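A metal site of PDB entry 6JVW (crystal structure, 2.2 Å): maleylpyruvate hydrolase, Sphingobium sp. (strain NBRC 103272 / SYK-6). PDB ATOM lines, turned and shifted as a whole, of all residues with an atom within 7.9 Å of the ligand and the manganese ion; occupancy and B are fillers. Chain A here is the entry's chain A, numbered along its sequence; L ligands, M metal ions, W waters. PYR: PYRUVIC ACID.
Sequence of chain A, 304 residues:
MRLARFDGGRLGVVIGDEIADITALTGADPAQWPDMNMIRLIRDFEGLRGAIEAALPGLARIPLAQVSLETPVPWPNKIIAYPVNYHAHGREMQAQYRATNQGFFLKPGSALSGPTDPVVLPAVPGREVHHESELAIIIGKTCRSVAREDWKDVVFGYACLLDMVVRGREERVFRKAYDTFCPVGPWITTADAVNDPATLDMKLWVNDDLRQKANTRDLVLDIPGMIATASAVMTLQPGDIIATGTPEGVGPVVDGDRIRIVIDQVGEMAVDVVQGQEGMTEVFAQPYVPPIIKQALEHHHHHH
O3 of the ligand lies close to NZ of Lys 176. N of Val 84 lies within hydrogen-bond range of O of the ligand, at 2.9 Å.
The side-chain carboxylate of Glu 134 is in hydrogen-bond range of the backbone NH of Gly 245, at 2.9 Å. The backbone NH of Glu 134 lies within hydrogen-bond range of the backbone carbonyl oxygen of Leu 161, 2.9 Å away. OD1 of Asp 163 lies within salt-bridge range of NZ of Lys 176, 3.4 Å away. The side-chain carboxylate (OD1) of Asp 163 is in salt-bridge range of the side-chain amino group (NZ) of Lys 107. O of Lys 176 lies within hydrogen-bond range of NZ of Lys 107, 2.9 Å away. N of Phe 105 sits at hydrogen-bond distance from O of Ala 81, at 2.8 Å. N of Tyr 82 sits at hydrogen-bond distance from O of Ala 243 (3.0 Å). The side-chain hydroxyl (OG1) of Thr 246 is in hydrogen-bond range of the backbone carbonyl oxygen (O) of Ser 133, at 2.9 Å.
O of Tyr 82 lies close to OXT of the ligand (3.3 Å). CA of Pro 83 touches C of the ligand (3.6 Å). CZ of Phe 105 touches O3 of the ligand, at 3.3 Å. Gly 245 touches the ligand (CA to OXT, 3.9 Å). Thr 246 touches the ligand. The nearest printed residue that does not touch the ligand is Ala 81 (5.4 Å).
Lys 176 touches the manganese ion. Of the 25 residues printed, 4 come within 4 Å of the manganese ion. Along chain A the residues within 4 Å of the manganese ion span positions 132 to 176. The nearest printed residue that does not touch the manganese ion is Tyr 82 (4.1 Å).
The manganese ion is bound by the side-chain carboxylate (OE2) of Glu 134 (2.0 Å). The manganese ion is bound by OD2 of Asp 163 (2.0 Å). An oxygen (OXT) of the ligand is bound to the manganese ion (2.1 Å). The manganese ion is bound by OE1 of Glu 132 (2.2 Å). The manganese ion is bound by water W1. O3 of the ligand binds the manganese ion, 2.3 Å away.
Water W1 bridges OE1 of Glu 134 (2.5 Å) and O of Tyr 82 (2.8 Å).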
ATOM      1  N   ALA A  81     -17.026  15.773 -21.685  1.00  0.00           N
ATOM      2  CA  ALA A  81     -16.402  15.541 -20.364  1.00  0.00           C
ATOM      3  C   ALA A  81     -15.577  16.780 -19.992  1.00  0.00           C
ATOM      4  O   ALA A  81     -14.853  17.333 -20.861  1.00  0.00           O
ATOM      5  CB  ALA A  81     -15.583  14.286 -20.372  1.00  0.00           C
ATOM      6  N   TYR A  82     -15.744  17.247 -18.764  1.00  0.00           N
ATOM      7  CA  TYR A  82     -14.959  18.375 -18.202  1.00  0.00           C
ATOM      8  C   TYR A  82     -13.793  17.818 -17.388  1.00  0.00           C
ATOM      9  O   TYR A  82     -13.963  17.009 -16.475  1.00  0.00           O
ATOM     10  CB  TYR A  82     -15.887  19.329 -17.472  1.00  0.00           C
ATOM     11  CG  TYR A  82     -16.715  20.173 -18.411  1.00  0.00           C
ATOM     12  CD1 TYR A  82     -16.248  21.384 -18.886  1.00  0.00           C
ATOM     13  CD2 TYR A  82     -17.979  19.756 -18.813  1.00  0.00           C
ATOM     14  CE1 TYR A  82     -17.011  22.173 -19.752  1.00  0.00           C
ATOM     15  CE2 TYR A  82     -18.753  20.532 -19.664  1.00  0.00           C
ATOM     16  CZ  TYR A  82     -18.278  21.748 -20.136  1.00  0.00           C
ATOM     17  OH  TYR A  82     -19.053  22.493 -20.967  1.00  0.00           O
ATOM     18  N   PRO A  83     -12.566  18.277 -17.700  1.00  0.00           N
ATOM     19  CA  PRO A  83     -11.393  17.822 -16.963  1.00  0.00           C
ATOM     20  C   PRO A  83     -11.319  18.587 -15.629  1.00  0.00           C
ATOM     21  O   PRO A  83     -11.656  19.754 -15.638  1.00  0.00           O
ATOM     22  CB  PRO A  83     -10.260  18.225 -17.917  1.00  0.00           C
ATOM     23  CG  PRO A  83     -10.750  19.537 -18.506  1.00  0.00           C
ATOM     24  CD  PRO A  83     -12.257  19.369 -18.634  1.00  0.00           C
ATOM     25  N   VAL A  84     -10.881  17.917 -14.561  1.00  0.00           N
ATOM     26  CA  VAL A  84     -10.611  18.450 -13.186  1.00  0.00           C
ATOM     27  C   VAL A  84     -11.976  18.767 -12.560  1.00  0.00           C
ATOM     28  O   VAL A  84     -12.696  17.784 -12.198  1.00  0.00           O
ATOM     29  CB  VAL A  84      -9.584  19.615 -13.176  1.00  0.00           C
ATOM     30  CG1 VAL A  84      -8.366  19.273 -14.026  1.00  0.00           C
ATOM     31  CG2 VAL A  84     -10.141  21.001 -13.549  1.00  0.00           C
ATOM     32  N   ASN A  85     -12.259  20.053 -12.364  1.00  0.00           N
ATOM     33  CA  ASN A  85     -13.592  20.657 -12.150  1.00  0.00           C
ATOM     34  C   ASN A  85     -14.057  20.463 -10.703  1.00  0.00           C
ATOM     35  O   ASN A  85     -15.263  20.682 -10.454  1.00  0.00           O
ATOM     36  CB  ASN A  85     -14.646  20.174 -13.160  1.00  0.00           C
ATOM     37  CG  ASN A  85     -15.681  21.249 -13.381  1.00  0.00           C
ATOM     38  OD1 ASN A  85     -15.324  22.425 -13.310  1.00  0.00           O
ATOM     39  ND2 ASN A  85     -16.954  20.876 -13.551  1.00  0.00           N
ATOM     40  N   TYR A  86     -13.157  20.135  -9.755  1.00  0.00           N
ATOM     41  CA  TYR A  86     -13.450  20.186  -8.297  1.00  0.00           C
ATOM     42  C   TYR A  86     -12.383  21.004  -7.542  1.00  0.00           C
ATOM     43  O   TYR A  86     -11.193  20.866  -7.804  1.00  0.00           O
ATOM     44  CB  TYR A  86     -13.558  18.785  -7.732  1.00  0.00           C
ATOM     45  CG  TYR A  86     -14.907  18.141  -7.944  1.00  0.00           C
ATOM     46  CD1 TYR A  86     -15.165  17.391  -9.079  1.00  0.00           C
ATOM     47  CD2 TYR A  86     -15.902  18.223  -6.985  1.00  0.00           C
ATOM     48  CE1 TYR A  86     -16.385  16.793  -9.288  1.00  0.00           C
ATOM     49  CE2 TYR A  86     -17.134  17.610  -7.170  1.00  0.00           C
ATOM     50  CZ  TYR A  86     -17.385  16.887  -8.336  1.00  0.00           C
ATOM     51  OH  TYR A  86     -18.571  16.250  -8.546  1.00  0.00           O
ATOM     52  N   PHE A 105     -13.612  17.866 -23.332  1.00  0.00           N
ATOM     53  CA  PHE A 105     -13.146  16.902 -24.363  1.00  0.00           C
ATOM     54  C   PHE A 105     -14.313  15.962 -24.670  1.00  0.00           C
ATOM     55  O   PHE A 105     -15.409  16.128 -24.103  1.00  0.00           O
ATOM     56  CB  PHE A 105     -11.835  16.247 -23.917  1.00  0.00           C
ATOM     57  CG  PHE A 105     -11.926  15.379 -22.693  1.00  0.00           C
ATOM     58  CD1 PHE A 105     -12.223  14.031 -22.803  1.00  0.00           C
ATOM     59  CD2 PHE A 105     -11.764  15.911 -21.418  1.00  0.00           C
ATOM     60  CE1 PHE A 105     -12.326  13.223 -21.675  1.00  0.00           C
ATOM     61  CE2 PHE A 105     -11.863  15.115 -20.285  1.00  0.00           C
ATOM     62  CZ  PHE A 105     -12.153  13.767 -20.416  1.00  0.00           C
ATOM     63  N   LYS A 107     -15.719  11.866 -25.391  1.00  0.00           N
ATOM     64  CA  LYS A 107     -15.543  10.395 -25.263  1.00  0.00           C
ATOM     65  C   LYS A 107     -16.368   9.770 -26.366  1.00  0.00           C
ATOM     66  O   LYS A 107     -17.451  10.273 -26.682  1.00  0.00           O
ATOM     67  CB  LYS A 107     -16.023   9.872 -23.906  1.00  0.00           C
ATOM     68  CG  LYS A 107     -15.277  10.397 -22.691  1.00  0.00           C
ATOM     69  CD  LYS A 107     -14.205   9.471 -22.156  1.00  0.00           C
ATOM     70  CE  LYS A 107     -14.744   8.457 -21.165  1.00  0.00           C
ATOM     71  NZ  LYS A 107     -13.650   7.583 -20.672  1.00  0.00           N
ATOM     72  N   HIS A 131      -9.348   5.138 -12.017  1.00  0.00           N
ATOM     73  CA  HIS A 131     -10.801   5.441 -11.841  1.00  0.00           C
ATOM     74  C   HIS A 131     -11.002   6.956 -11.727  1.00  0.00           C
ATOM     75  O   HIS A 131     -10.089   7.659 -11.276  1.00  0.00           O
ATOM     76  CB  HIS A 131     -11.401   4.723 -10.621  1.00  0.00           C
ATOM     77  CG  HIS A 131     -10.820   5.207  -9.346  1.00  0.00           C
ATOM     78  ND1 HIS A 131      -9.908   4.447  -8.612  1.00  0.00           N
ATOM     79  CD2 HIS A 131     -10.904   6.400  -8.716  1.00  0.00           C
ATOM     80  CE1 HIS A 131      -9.498   5.154  -7.573  1.00  0.00           C
ATOM     81  NE2 HIS A 131     -10.098   6.345  -7.617  1.00  0.00           N
ATOM     82  N   GLU A 132     -12.162   7.430 -12.151  1.00  0.00           N
ATOM     83  CA  GLU A 132     -12.654   8.809 -11.976  1.00  0.00           C
ATOM     84  C   GLU A 132     -14.175   8.736 -11.732  1.00  0.00           C
ATOM     85  O   GLU A 132     -14.895   8.340 -12.675  1.00  0.00           O
ATOM     86  CB  GLU A 132     -12.401   9.654 -13.222  1.00  0.00           C
ATOM     87  CG  GLU A 132     -10.939   9.917 -13.561  1.00  0.00           C
ATOM     88  CD  GLU A 132     -10.785  10.958 -14.654  1.00  0.00           C
ATOM     89  OE1 GLU A 132     -11.835  11.458 -15.129  1.00  0.00           O
ATOM     90  OE2 GLU A 132      -9.630  11.270 -15.044  1.00  0.00           O
ATOM     91  N   SER A 133     -14.635   9.082 -10.535  1.00  0.00           N
ATOM     92  CA  SER A 133     -16.071   9.125 -10.168  1.00  0.00           C
ATOM     93  C   SER A 133     -16.623  10.466 -10.623  1.00  0.00           C
ATOM     94  O   SER A 133     -15.970  11.482 -10.329  1.00  0.00           O
ATOM     95  CB  SER A 133     -16.302   8.935  -8.679  1.00  0.00           C
ATOM     96  OG  SER A 133     -15.641   9.940  -7.944  1.00  0.00           O
ATOM     97  N   GLU A 134     -17.736  10.442 -11.327  1.00  0.00           N
ATOM     98  CA  GLU A 134     -18.357  11.672 -11.890  1.00  0.00           C
ATOM     99  C   GLU A 134     -19.895  11.573 -11.831  1.00  0.00           C
ATOM    100  O   GLU A 134     -20.488  10.486 -12.048  1.00  0.00           O
ATOM    101  CB  GLU A 134     -17.852  11.938 -13.324  1.00  0.00           C
ATOM    102  CG  GLU A 134     -16.342  11.829 -13.524  1.00  0.00           C
ATOM    103  CD  GLU A 134     -15.699  12.609 -14.692  1.00  0.00           C
ATOM    104  OE1 GLU A 134     -16.366  13.420 -15.352  1.00  0.00           O
ATOM    105  OE2 GLU A 134     -14.472  12.445 -14.916  1.00  0.00           O
ATOM    106  N   LEU A 161     -21.269   7.954 -13.366  1.00  0.00           N
ATOM    107  CA  LEU A 161     -20.330   7.751 -14.489  1.00  0.00           C
ATOM    108  C   LEU A 161     -18.919   7.498 -13.934  1.00  0.00           C
ATOM    109  O   LEU A 161     -18.512   8.129 -12.936  1.00  0.00           O
ATOM    110  CB  LEU A 161     -20.386   8.989 -15.389  1.00  0.00           C
ATOM    111  CG  LEU A 161     -19.514   8.940 -16.631  1.00  0.00           C
ATOM    112  CD1 LEU A 161     -20.195   9.648 -17.779  1.00  0.00           C
ATOM    113  CD2 LEU A 161     -18.124   9.547 -16.375  1.00  0.00           C
ATOM    114  N   LEU A 162     -18.221   6.540 -14.543  1.00  0.00           N
ATOM    115  CA  LEU A 162     -16.783   6.306 -14.302  1.00  0.00           C
ATOM    116  C   LEU A 162     -16.015   6.736 -15.552  1.00  0.00           C
ATOM    117  O   LEU A 162     -16.256   6.148 -16.577  1.00  0.00           O
ATOM    118  CB  LEU A 162     -16.583   4.829 -13.990  1.00  0.00           C
ATOM    119  CG  LEU A 162     -17.205   4.351 -12.676  1.00  0.00           C
ATOM    120  CD1 LEU A 162     -17.032   2.841 -12.510  1.00  0.00           C
ATOM    121  CD2 LEU A 162     -16.595   5.110 -11.504  1.00  0.00           C
ATOM    122  N   ASP A 163     -15.120   7.708 -15.440  1.00  0.00           N
ATOM    123  CA  ASP A 163     -14.321   8.209 -16.581  1.00  0.00           C
ATOM    124  C   ASP A 163     -12.954   7.540 -16.480  1.00  0.00           C
ATOM    125  O   ASP A 163     -12.011   8.193 -16.002  1.00  0.00           O
ATOM    126  CB  ASP A 163     -14.316   9.748 -16.583  1.00  0.00           C
ATOM    127  CG  ASP A 163     -13.547  10.391 -17.725  1.00  0.00           C
ATOM    128  OD1 ASP A 163     -13.245   9.676 -18.710  1.00  0.00           O
ATOM    129  OD2 ASP A 163     -13.220  11.602 -17.589  1.00  0.00           O
ATOM    130  N   MET A 164     -12.844   6.294 -16.964  1.00  0.00           N
ATOM    131  CA  MET A 164     -11.595   5.481 -16.849  1.00  0.00           C
ATOM    132  C   MET A 164     -10.548   5.996 -17.834  1.00  0.00           C
ATOM    133  O   MET A 164     -10.908   6.369 -18.934  1.00  0.00           O
ATOM    134  CB  MET A 164     -11.856   4.000 -17.128  1.00  0.00           C
ATOM    135  CG  MET A 164     -12.991   3.401 -16.340  1.00  0.00           C
ATOM    136  SD  MET A 164     -12.867   3.549 -14.519  1.00  0.00           S
ATOM    137  CE  MET A 164     -11.451   2.490 -14.221  1.00  0.00           C
ATOM    138  N   VAL A 165      -9.281   6.024 -17.445  1.00  0.00           N
ATOM    139  CA  VAL A 165      -8.172   6.570 -18.279  1.00  0.00           C
ATOM    140  C   VAL A 165      -6.868   5.777 -18.074  1.00  0.00           C
ATOM    141  O   VAL A 165      -6.549   5.421 -16.917  1.00  0.00           O
ATOM    142  CB  VAL A 165      -7.968   8.058 -17.984  1.00  0.00           C
ATOM    143  CG1 VAL A 165      -7.673   8.322 -16.529  1.00  0.00           C
ATOM    144  CG2 VAL A 165      -6.864   8.639 -18.859  1.00  0.00           C
ATOM    145  N   ARG A 167      -3.093   6.136 -17.679  1.00  0.00           N
ATOM    146  CA  ARG A 167      -2.375   7.314 -17.139  1.00  0.00           C
ATOM    147  C   ARG A 167      -1.131   7.614 -18.011  1.00  0.00           C
ATOM    148  O   ARG A 167      -0.468   6.652 -18.442  1.00  0.00           O
ATOM    149  CB  ARG A 167      -2.063   7.134 -15.653  1.00  0.00           C
ATOM    150  CG  ARG A 167      -1.626   8.403 -14.928  1.00  0.00           C
ATOM    151  CD  ARG A 167      -2.221   9.715 -15.455  1.00  0.00           C
ATOM    152  NE  ARG A 167      -3.671   9.788 -15.370  1.00  0.00           N
ATOM    153  CZ  ARG A 167      -4.337  10.173 -14.292  1.00  0.00           C
ATOM    154  NH1 ARG A 167      -3.697  10.528 -13.191  1.00  0.00           N
ATOM    155  NH2 ARG A 167      -5.662  10.214 -14.313  1.00  0.00           N
ATOM    156  N   LYS A 176      -8.482   7.804 -23.128  1.00  0.00           N
ATOM    157  CA  LYS A 176      -9.829   7.851 -22.510  1.00  0.00           C
ATOM    158  C   LYS A 176     -10.845   7.102 -23.382  1.00  0.00           C
ATOM    159  O   LYS A 176     -12.027   7.055 -22.987  1.00  0.00           O
ATOM    160  CB  LYS A 176     -10.289   9.297 -22.326  1.00  0.00           C
ATOM    161  CG  LYS A 176      -9.284  10.189 -21.614  1.00  0.00           C
ATOM    162  CD  LYS A 176      -9.886  11.129 -20.599  1.00  0.00           C
ATOM    163  CE  LYS A 176     -10.197  10.440 -19.298  1.00  0.00           C
ATOM    164  NZ  LYS A 176     -10.398  11.390 -18.184  1.00  0.00           N
ATOM    165  N   ALA A 243     -20.267  14.530 -18.536  1.00  0.00           N
ATOM    166  CA  ALA A 243     -19.422  14.088 -17.424  1.00  0.00           C
ATOM    167  C   ALA A 243     -18.880  15.336 -16.726  1.00  0.00           C
ATOM    168  O   ALA A 243     -18.162  16.059 -17.365  1.00  0.00           O
ATOM    169  CB  ALA A 243     -18.344  13.222 -18.002  1.00  0.00           C
ATOM    170  N   THR A 244     -19.253  15.599 -15.475  1.00  0.00           N
ATOM    171  CA  THR A 244     -19.058  16.938 -14.850  1.00  0.00           C
ATOM    172  C   THR A 244     -17.677  17.096 -14.167  1.00  0.00           C
ATOM    173  O   THR A 244     -17.410  18.191 -13.674  1.00  0.00           O
ATOM    174  CB  THR A 244     -20.231  17.209 -13.914  1.00  0.00           C
ATOM    175  OG1 THR A 244     -20.201  16.096 -13.033  1.00  0.00           O
ATOM    176  CG2 THR A 244     -21.549  17.321 -14.654  1.00  0.00           C
ATOM    177  N   GLY A 245     -16.833  16.056 -14.173  1.00  0.00           N
ATOM    178  CA  GLY A 245     -15.485  16.072 -13.583  1.00  0.00           C
ATOM    179  C   GLY A 245     -15.361  15.130 -12.383  1.00  0.00           C
ATOM    180  O   GLY A 245     -16.342  14.526 -12.000  1.00  0.00           O
ATOM    181  N   THR A 246     -14.158  15.003 -11.837  1.00  0.00           N
ATOM    182  CA  THR A 246     -13.817  14.073 -10.734  1.00  0.00           C
ATOM    183  C   THR A 246     -13.051  14.861  -9.682  1.00  0.00           C
ATOM    184  O   THR A 246     -12.349  15.808 -10.006  1.00  0.00           O
ATOM    185  CB  THR A 246     -13.022  12.874 -11.276  1.00  0.00           C
ATOM    186  OG1 THR A 246     -13.114  11.769 -10.363  1.00  0.00           O
ATOM    187  CG2 THR A 246     -11.586  13.239 -11.566  1.00  0.00           C
ATOM    188  N   PRO A 247     -13.220  14.549  -8.386  1.00  0.00           N
ATOM    189  CA  PRO A 247     -12.378  15.175  -7.367  1.00  0.00           C
ATOM    190  C   PRO A 247     -11.029  14.444  -7.185  1.00  0.00           C
ATOM    191  O   PRO A 247     -10.734  13.550  -7.972  1.00  0.00           O
ATOM    192  CB  PRO A 247     -13.309  15.106  -6.147  1.00  0.00           C
ATOM    193  CG  PRO A 247     -14.045  13.805  -6.337  1.00  0.00           C
ATOM    194  CD  PRO A 247     -14.274  13.706  -7.826  1.00  0.00           C
ATOM    195  N   VAL A 250      -8.026  10.166  -7.421  1.00  0.00           N
ATOM    196  CA  VAL A 250      -7.888   9.385  -8.691  1.00  0.00           C
ATOM    197  C   VAL A 250      -6.712   8.434  -8.489  1.00  0.00           C
ATOM    198  O   VAL A 250      -5.645   8.903  -8.112  1.00  0.00           O
ATOM    199  CB  VAL A 250      -7.670  10.320  -9.906  1.00  0.00           C
ATOM    200  CG1 VAL A 250      -7.242   9.533 -11.142  1.00  0.00           C
ATOM    201  CG2 VAL A 250      -8.899  11.170 -10.209  1.00  0.00           C
HETATM  202  C   PYR L   1     -10.985  14.630 -15.336  1.00  0.00           C
HETATM  203  O   PYR L   1     -10.170  15.153 -14.557  1.00  0.00           O
HETATM  204  OXT PYR L   1     -12.235  14.589 -15.099  1.00  0.00           O
HETATM  205  CA  PYR L   1     -10.441  14.137 -16.440  1.00  0.00           C
HETATM  206  O3  PYR L   1     -11.166  13.614 -17.305  1.00  0.00           O
HETATM  207  CB  PYR L   1      -8.959  14.200 -16.694  1.00  0.00           C
HETATM  208 MN    MN M   1     -13.034  12.986 -16.145  1.00  0.00          MN
HETATM  209  O   HOH W   1     -14.598  14.364 -16.898  1.00  0.00           O
